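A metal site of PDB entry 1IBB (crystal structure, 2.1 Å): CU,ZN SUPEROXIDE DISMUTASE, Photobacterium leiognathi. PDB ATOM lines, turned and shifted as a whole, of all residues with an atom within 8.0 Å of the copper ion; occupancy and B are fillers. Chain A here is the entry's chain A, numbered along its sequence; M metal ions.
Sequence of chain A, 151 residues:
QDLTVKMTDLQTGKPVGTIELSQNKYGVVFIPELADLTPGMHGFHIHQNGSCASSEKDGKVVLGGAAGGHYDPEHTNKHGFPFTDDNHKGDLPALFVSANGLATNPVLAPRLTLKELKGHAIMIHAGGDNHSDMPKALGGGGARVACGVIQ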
ATOM      1  N   GLY A  43       8.699 -29.613  -9.965  1.00  0.00           N
ATOM      2  CA  GLY A  43       7.466 -29.471 -10.721  1.00  0.00           C
ATOM      3  C   GLY A  43       6.677 -28.392 -10.014  1.00  0.00           C
ATOM      4  O   GLY A  43       6.546 -28.404  -8.785  1.00  0.00           O
ATOM      5  N   PHE A  44       6.121 -27.469 -10.794  1.00  0.00           N
ATOM      6  CA  PHE A  44       5.400 -26.336 -10.244  1.00  0.00           C
ATOM      7  C   PHE A  44       4.138 -26.132 -11.051  1.00  0.00           C
ATOM      8  O   PHE A  44       4.194 -25.763 -12.222  1.00  0.00           O
ATOM      9  CB  PHE A  44       6.346 -25.140 -10.365  1.00  0.00           C
ATOM     10  CG  PHE A  44       5.914 -23.922  -9.609  1.00  0.00           C
ATOM     11  CD1 PHE A  44       5.310 -24.038  -8.367  1.00  0.00           C
ATOM     12  CD2 PHE A  44       6.183 -22.662 -10.116  1.00  0.00           C
ATOM     13  CE1 PHE A  44       4.982 -22.906  -7.634  1.00  0.00           C
ATOM     14  CE2 PHE A  44       5.856 -21.528  -9.400  1.00  0.00           C
ATOM     15  CZ  PHE A  44       5.259 -21.649  -8.153  1.00  0.00           C
ATOM     16  N   HIS A  45       2.986 -26.379 -10.438  1.00  0.00           N
ATOM     17  CA  HIS A  45       1.716 -26.213 -11.146  1.00  0.00           C
ATOM     18  C   HIS A  45       0.580 -25.693 -10.309  1.00  0.00           C
ATOM     19  O   HIS A  45       0.594 -25.788  -9.077  1.00  0.00           O
ATOM     20  CB  HIS A  45       1.214 -27.533 -11.756  1.00  0.00           C
ATOM     21  CG  HIS A  45       2.284 -28.550 -12.015  1.00  0.00           C
ATOM     22  ND1 HIS A  45       2.540 -29.588 -11.149  1.00  0.00           N
ATOM     23  CD2 HIS A  45       3.113 -28.728 -13.074  1.00  0.00           C
ATOM     24  CE1 HIS A  45       3.477 -30.358 -11.655  1.00  0.00           C
ATOM     25  NE2 HIS A  45       3.842 -29.863 -12.822  1.00  0.00           N
ATOM     26  N   ILE A  46      -0.422 -25.159 -10.993  1.00  0.00           N
ATOM     27  CA  ILE A  46      -1.626 -24.676 -10.365  1.00  0.00           C
ATOM     28  C   ILE A  46      -2.587 -25.851 -10.441  1.00  0.00           C
ATOM     29  O   ILE A  46      -2.765 -26.452 -11.510  1.00  0.00           O
ATOM     30  CB  ILE A  46      -2.260 -23.522 -11.128  1.00  0.00           C
ATOM     31  CG1 ILE A  46      -1.319 -22.307 -11.153  1.00  0.00           C
ATOM     32  CG2 ILE A  46      -3.596 -23.153 -10.484  1.00  0.00           C
ATOM     33  CD1 ILE A  46      -1.055 -21.725  -9.771  1.00  0.00           C
ATOM     34  N   HIS A  47      -3.186 -26.211  -9.305  1.00  0.00           N
ATOM     35  CA  HIS A  47      -4.132 -27.327  -9.254  1.00  0.00           C
ATOM     36  C   HIS A  47      -5.591 -26.853  -9.216  1.00  0.00           C
ATOM     37  O   HIS A  47      -5.858 -25.709  -8.887  1.00  0.00           O
ATOM     38  CB  HIS A  47      -3.818 -28.216  -8.064  1.00  0.00           C
ATOM     39  CG  HIS A  47      -2.712 -29.188  -8.326  1.00  0.00           C
ATOM     40  ND1 HIS A  47      -2.906 -30.554  -8.314  1.00  0.00           N
ATOM     41  CD2 HIS A  47      -1.404 -28.997  -8.615  1.00  0.00           C
ATOM     42  CE1 HIS A  47      -1.770 -31.161  -8.597  1.00  0.00           C
ATOM     43  NE2 HIS A  47      -0.838 -30.231  -8.786  1.00  0.00           N
ATOM     44  N   ALA A  67      -6.223 -31.206  -3.429  1.00  0.00           N
ATOM     45  CA  ALA A  67      -6.038 -30.156  -4.428  1.00  0.00           C
ATOM     46  C   ALA A  67      -6.518 -30.604  -5.811  1.00  0.00           C
ATOM     47  O   ALA A  67      -6.716 -29.774  -6.703  1.00  0.00           O
ATOM     48  CB  ALA A  67      -4.566 -29.747  -4.494  1.00  0.00           C
ATOM     49  N   GLY A  68      -6.705 -31.914  -5.990  1.00  0.00           N
ATOM     50  CA  GLY A  68      -7.157 -32.414  -7.273  1.00  0.00           C
ATOM     51  C   GLY A  68      -6.039 -32.416  -8.293  1.00  0.00           C
ATOM     52  O   GLY A  68      -4.866 -32.335  -7.947  1.00  0.00           O
ATOM     53  N   GLY A  69      -6.412 -32.502  -9.575  1.00  0.00           N
ATOM     54  CA  GLY A  69      -5.420 -32.518 -10.641  1.00  0.00           C
ATOM     55  C   GLY A  69      -4.968 -31.123 -11.040  1.00  0.00           C
ATOM     56  O   GLY A  69      -5.176 -30.163 -10.283  1.00  0.00           O
ATOM     57  N   HIS A  70      -4.347 -31.006 -12.210  1.00  0.00           N
ATOM     58  CA  HIS A  70      -3.865 -29.713 -12.704  1.00  0.00           C
ATOM     59  C   HIS A  70      -4.990 -28.847 -13.260  1.00  0.00           C
ATOM     60  O   HIS A  70      -5.890 -29.351 -13.925  1.00  0.00           O
ATOM     61  CB  HIS A  70      -2.808 -29.918 -13.787  1.00  0.00           C
ATOM     62  CG  HIS A  70      -1.504 -30.455 -13.282  1.00  0.00           C
ATOM     63  ND1 HIS A  70      -0.451 -30.747 -14.115  1.00  0.00           N
ATOM     64  CD2 HIS A  70      -1.095 -30.766 -12.032  1.00  0.00           C
ATOM     65  CE1 HIS A  70       0.558 -31.216 -13.398  1.00  0.00           C
ATOM     66  NE2 HIS A  70       0.190 -31.231 -12.126  1.00  0.00           N
ATOM     67  N   TYR A  71      -4.922 -27.555 -12.993  1.00  0.00           N
ATOM     68  CA  TYR A  71      -5.913 -26.608 -13.487  1.00  0.00           C
ATOM     69  C   TYR A  71      -5.978 -26.832 -15.009  1.00  0.00           C
ATOM     70  O   TYR A  71      -4.961 -26.738 -15.712  1.00  0.00           O
ATOM     71  CB  TYR A  71      -5.461 -25.180 -13.151  1.00  0.00           C
ATOM     72  CG  TYR A  71      -6.369 -24.068 -13.628  1.00  0.00           C
ATOM     73  CD1 TYR A  71      -7.728 -24.042 -13.293  1.00  0.00           C
ATOM     74  CD2 TYR A  71      -5.865 -23.025 -14.397  1.00  0.00           C
ATOM     75  CE1 TYR A  71      -8.556 -22.989 -13.720  1.00  0.00           C
ATOM     76  CE2 TYR A  71      -6.679 -21.980 -14.831  1.00  0.00           C
ATOM     77  CZ  TYR A  71      -8.010 -21.964 -14.483  1.00  0.00           C
ATOM     78  OH  TYR A  71      -8.795 -20.910 -14.925  1.00  0.00           O
ATOM     79  N   HIS A  79      -0.673 -32.872 -20.231  1.00  0.00           N
ATOM     80  CA  HIS A  79       0.270 -32.054 -19.490  1.00  0.00           C
ATOM     81  C   HIS A  79       1.312 -31.590 -20.494  1.00  0.00           C
ATOM     82  O   HIS A  79       1.752 -32.366 -21.338  1.00  0.00           O
ATOM     83  CB  HIS A  79       0.916 -32.868 -18.373  1.00  0.00           C
ATOM     84  CG  HIS A  79       2.013 -32.144 -17.646  1.00  0.00           C
ATOM     85  ND1 HIS A  79       1.765 -31.179 -16.692  1.00  0.00           N
ATOM     86  CD2 HIS A  79       3.360 -32.262 -17.727  1.00  0.00           C
ATOM     87  CE1 HIS A  79       2.916 -30.727 -16.229  1.00  0.00           C
ATOM     88  NE2 HIS A  79       3.893 -31.367 -16.843  1.00  0.00           N
ATOM     89  N   HIS A  88      -2.871 -28.588 -19.906  1.00  0.00           N
ATOM     90  CA  HIS A  88      -3.253 -27.903 -18.675  1.00  0.00           C
ATOM     91  C   HIS A  88      -2.777 -26.456 -18.620  1.00  0.00           C
ATOM     92  O   HIS A  88      -1.589 -26.186 -18.749  1.00  0.00           O
ATOM     93  CB  HIS A  88      -2.672 -28.619 -17.460  1.00  0.00           C
ATOM     94  CG  HIS A  88      -2.949 -30.082 -17.421  1.00  0.00           C
ATOM     95  ND1 HIS A  88      -1.993 -31.010 -17.049  1.00  0.00           N
ATOM     96  CD2 HIS A  88      -4.082 -30.784 -17.650  1.00  0.00           C
ATOM     97  CE1 HIS A  88      -2.534 -32.209 -17.048  1.00  0.00           C
ATOM     98  NE2 HIS A  88      -3.799 -32.104 -17.402  1.00  0.00           N
ATOM     99  N   GLY A  90      -2.693 -24.917 -16.100  1.00  0.00           N
ATOM    100  CA  GLY A  90      -2.044 -24.796 -14.806  1.00  0.00           C
ATOM    101  C   GLY A  90      -0.573 -25.166 -14.851  1.00  0.00           C
ATOM    102  O   GLY A  90       0.112 -25.100 -13.832  1.00  0.00           O
ATOM    103  N   ASP A  91      -0.091 -25.543 -16.026  1.00  0.00           N
ATOM    104  CA  ASP A  91       1.308 -25.929 -16.200  1.00  0.00           C
ATOM    105  C   ASP A  91       2.214 -24.694 -16.219  1.00  0.00           C
ATOM    106  O   ASP A  91       2.130 -23.863 -17.139  1.00  0.00           O
ATOM    107  CB  ASP A  91       1.469 -26.744 -17.489  1.00  0.00           C
ATOM    108  CG  ASP A  91       0.694 -28.040 -17.447  1.00  0.00           C
ATOM    109  OD1 ASP A  91       0.466 -28.545 -16.325  1.00  0.00           O
ATOM    110  OD2 ASP A  91       0.313 -28.576 -18.503  1.00  0.00           O
ATOM    111  N   ALA A 121      -5.138 -24.022  -5.900  1.00  0.00           N
ATOM    112  CA  ALA A 121      -3.965 -24.315  -5.088  1.00  0.00           C
ATOM    113  C   ALA A 121      -2.681 -24.305  -5.914  1.00  0.00           C
ATOM    114  O   ALA A 121      -2.664 -24.743  -7.064  1.00  0.00           O
ATOM    115  CB  ALA A 121      -4.134 -25.677  -4.413  1.00  0.00           C
ATOM    116  N   ILE A 122      -1.598 -23.790  -5.330  1.00  0.00           N
ATOM    117  CA  ILE A 122      -0.309 -23.762  -6.001  1.00  0.00           C
ATOM    118  C   ILE A 122       0.440 -24.963  -5.419  1.00  0.00           C
ATOM    119  O   ILE A 122       0.525 -25.099  -4.199  1.00  0.00           O
ATOM    120  CB  ILE A 122       0.487 -22.482  -5.705  1.00  0.00           C
ATOM    121  CG1 ILE A 122      -0.275 -21.260  -6.179  1.00  0.00           C
ATOM    122  CG2 ILE A 122       1.853 -22.553  -6.414  1.00  0.00           C
ATOM    123  CD1 ILE A 122       0.392 -19.934  -5.832  1.00  0.00           C
ATOM    124  N   MET A 123       0.970 -25.817  -6.279  1.00  0.00           N
ATOM    125  CA  MET A 123       1.679 -27.001  -5.832  1.00  0.00           C
ATOM    126  C   MET A 123       3.147 -27.044  -6.221  1.00  0.00           C
ATOM    127  O   MET A 123       3.533 -26.558  -7.277  1.00  0.00           O
ATOM    128  CB  MET A 123       1.022 -28.255  -6.413  1.00  0.00           C
ATOM    129  CG  MET A 123       1.266 -29.504  -5.602  1.00  0.00           C
ATOM    130  SD  MET A 123       0.429 -29.421  -4.008  1.00  0.00           S
ATOM    131  CE  MET A 123      -1.206 -29.654  -4.436  1.00  0.00           C
ATOM    132  N   ILE A 124       3.958 -27.652  -5.361  1.00  0.00           N
ATOM    133  CA  ILE A 124       5.378 -27.825  -5.615  1.00  0.00           C
ATOM    134  C   ILE A 124       5.599 -29.320  -5.402  1.00  0.00           C
ATOM    135  O   ILE A 124       5.226 -29.862  -4.359  1.00  0.00           O
ATOM    136  CB  ILE A 124       6.254 -27.048  -4.614  1.00  0.00           C
ATOM    137  CG1 ILE A 124       6.076 -25.537  -4.828  1.00  0.00           C
ATOM    138  CG2 ILE A 124       7.718 -27.431  -4.790  1.00  0.00           C
ATOM    139  CD1 ILE A 124       6.767 -24.688  -3.777  1.00  0.00           C
ATOM    140  N   HIS A 125       6.180 -29.972  -6.388  1.00  0.00           N
ATOM    141  CA  HIS A 125       6.421 -31.398  -6.334  1.00  0.00           C
ATOM    142  C   HIS A 125       7.845 -31.766  -5.960  1.00  0.00           C
ATOM    143  O   HIS A 125       8.753 -30.926  -6.042  1.00  0.00           O
ATOM    144  CB  HIS A 125       6.087 -32.055  -7.667  1.00  0.00           C
ATOM    145  CG  HIS A 125       4.636 -31.995  -8.022  1.00  0.00           C
ATOM    146  ND1 HIS A 125       3.839 -33.115  -8.079  1.00  0.00           N
ATOM    147  CD2 HIS A 125       3.834 -30.944  -8.302  1.00  0.00           C
ATOM    148  CE1 HIS A 125       2.601 -32.759  -8.378  1.00  0.00           C
ATOM    149  NE2 HIS A 125       2.574 -31.449  -8.523  1.00  0.00           N
ATOM    150  N   ASP A 129      10.013 -31.672 -13.884  1.00  0.00           N
ATOM    151  CA  ASP A 129       8.934 -31.536 -14.847  1.00  0.00           C
ATOM    152  C   ASP A 129       9.492 -31.425 -16.273  1.00  0.00           C
ATOM    153  O   ASP A 129      10.049 -30.398 -16.631  1.00  0.00           O
ATOM    154  CB  ASP A 129       8.111 -30.289 -14.521  1.00  0.00           C
ATOM    155  CG  ASP A 129       6.806 -30.210 -15.285  1.00  0.00           C
ATOM    156  OD1 ASP A 129       6.622 -30.996 -16.247  1.00  0.00           O
ATOM    157  OD2 ASP A 129       5.959 -29.357 -14.937  1.00  0.00           O
ATOM    158  N   LEU A 138       2.246 -36.458 -15.977  1.00  0.00           N
ATOM    159  CA  LEU A 138       2.360 -35.177 -15.304  1.00  0.00           C
ATOM    160  C   LEU A 138       3.804 -34.698 -15.198  1.00  0.00           C
ATOM    161  O   LEU A 138       4.199 -34.092 -14.201  1.00  0.00           O
ATOM    162  CB  LEU A 138       1.734 -35.273 -13.909  1.00  0.00           C
ATOM    163  CG  LEU A 138       0.314 -35.844 -13.875  1.00  0.00           C
ATOM    164  CD1 LEU A 138      -0.221 -35.723 -12.460  1.00  0.00           C
ATOM    165  CD2 LEU A 138      -0.585 -35.109 -14.856  1.00  0.00           C
ATOM    166  N   GLY A 141       6.597 -35.114 -11.813  1.00  0.00           N
ATOM    167  CA  GLY A 141       6.698 -34.397 -10.562  1.00  0.00           C
ATOM    168  C   GLY A 141       6.569 -35.294  -9.344  1.00  0.00           C
ATOM    169  O   GLY A 141       7.105 -34.983  -8.282  1.00  0.00           O
ATOM    170  N   GLY A 142       5.834 -36.397  -9.477  1.00  0.00           N
ATOM    171  CA  GLY A 142       5.662 -37.300  -8.356  1.00  0.00           C
ATOM    172  C   GLY A 142       4.946 -36.688  -7.157  1.00  0.00           C
ATOM    173  O   GLY A 142       3.992 -35.936  -7.315  1.00  0.00           O
ATOM    174  N   ALA A 143       5.407 -37.015  -5.946  1.00  0.00           N
ATOM    175  CA  ALA A 143       4.779 -36.511  -4.733  1.00  0.00           C
ATOM    176  C   ALA A 143       4.718 -34.992  -4.663  1.00  0.00           C
ATOM    177  O   ALA A 143       5.499 -34.289  -5.299  1.00  0.00           O
ATOM    178  CB  ALA A 143       5.522 -37.041  -3.522  1.00  0.00           C
ATOM    179  N   ARG A 144       3.767 -34.502  -3.877  1.00  0.00           N
ATOM    180  CA  ARG A 144       3.568 -33.067  -3.664  1.00  0.00           C
ATOM    181  C   ARG A 144       4.246 -32.713  -2.353  1.00  0.00           C
ATOM    182  O   ARG A 144       3.893 -33.269  -1.311  1.00  0.00           O
ATOM    183  CB  ARG A 144       2.079 -32.774  -3.597  1.00  0.00           C
ATOM    184  CG  ARG A 144       1.343 -33.230  -4.846  1.00  0.00           C
ATOM    185  CD  ARG A 144      -0.098 -33.612  -4.575  1.00  0.00           C
ATOM    186  NE  ARG A 144      -0.732 -34.106  -5.781  1.00  0.00           N
ATOM    187  CZ  ARG A 144      -1.933 -33.741  -6.205  1.00  0.00           C
ATOM    188  NH1 ARG A 144      -2.637 -32.864  -5.516  1.00  0.00           N
ATOM    189  NH2 ARG A 144      -2.430 -34.243  -7.327  1.00  0.00           N
ATOM    190  N   ALA A 146       5.060 -29.172  -1.300  1.00  0.00           N
ATOM    191  CA  ALA A 146       4.605 -27.913  -0.732  1.00  0.00           C
ATOM    192  C   ALA A 146       3.347 -27.435  -1.436  1.00  0.00           C
ATOM    193  O   ALA A 146       3.187 -27.600  -2.645  1.00  0.00           O
ATOM    194  CB  ALA A 146       5.708 -26.852  -0.839  1.00  0.00           C
HETATM  195 CU    CU M   1       1.171 -30.402  -9.755  1.00  0.00          CU
HETATM  196 ZN    ZN M   2      -0.186 -30.294 -16.125  1.00  0.00          ZN
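Met 123 touches the copper ion (CB to CU, 3.98 Å).
Of the 26 residues printed, 5 come within 4 Å of the copper ion.
O of Gly 68 sits at hydrogen-bond distance from ND1 of His 47.
O of Gly 43 sits at hydrogen-bond distance from N of His 125.
The backbone carbonyl oxygen (O) of Ala 143 lies close to a ring nitrogen (ND1) of His 125, at 3.4 Å.
ND1 of His 125 is in hydrogen-bond range of O of Gly 142 (2.9 Å).
The backbone carbonyl oxygen (O) of Ala 121 lies within hydrogen-bond range of the backbone NH (N) of His 47 (2.7 Å).
A ring nitrogen (ND1) of His 47 is in hydrogen-bond range of the backbone carbonyl oxygen (O) of Gly 69 (3.0 Å).
A ring nitrogen (NE2) of His 45 sits at hydrogen-bond distance from the side-chain carboxylate (OD2) of Asp 129, 3.0 Å away.
A ring nitrogen (ND1) of His 45 lies close to a ring nitrogen (NE2) of His 70 (3.0 Å).
The copper ion is bound by a ring nitrogen (ND1) of His 45, a ring nitrogen (NE2) of His 125 and a ring nitrogen (NE2) of His 47.
The copper ion has three donor atoms within binding distance.
Slightly farther from the copper ion lies NE2 of His 70 (2.7 Å).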
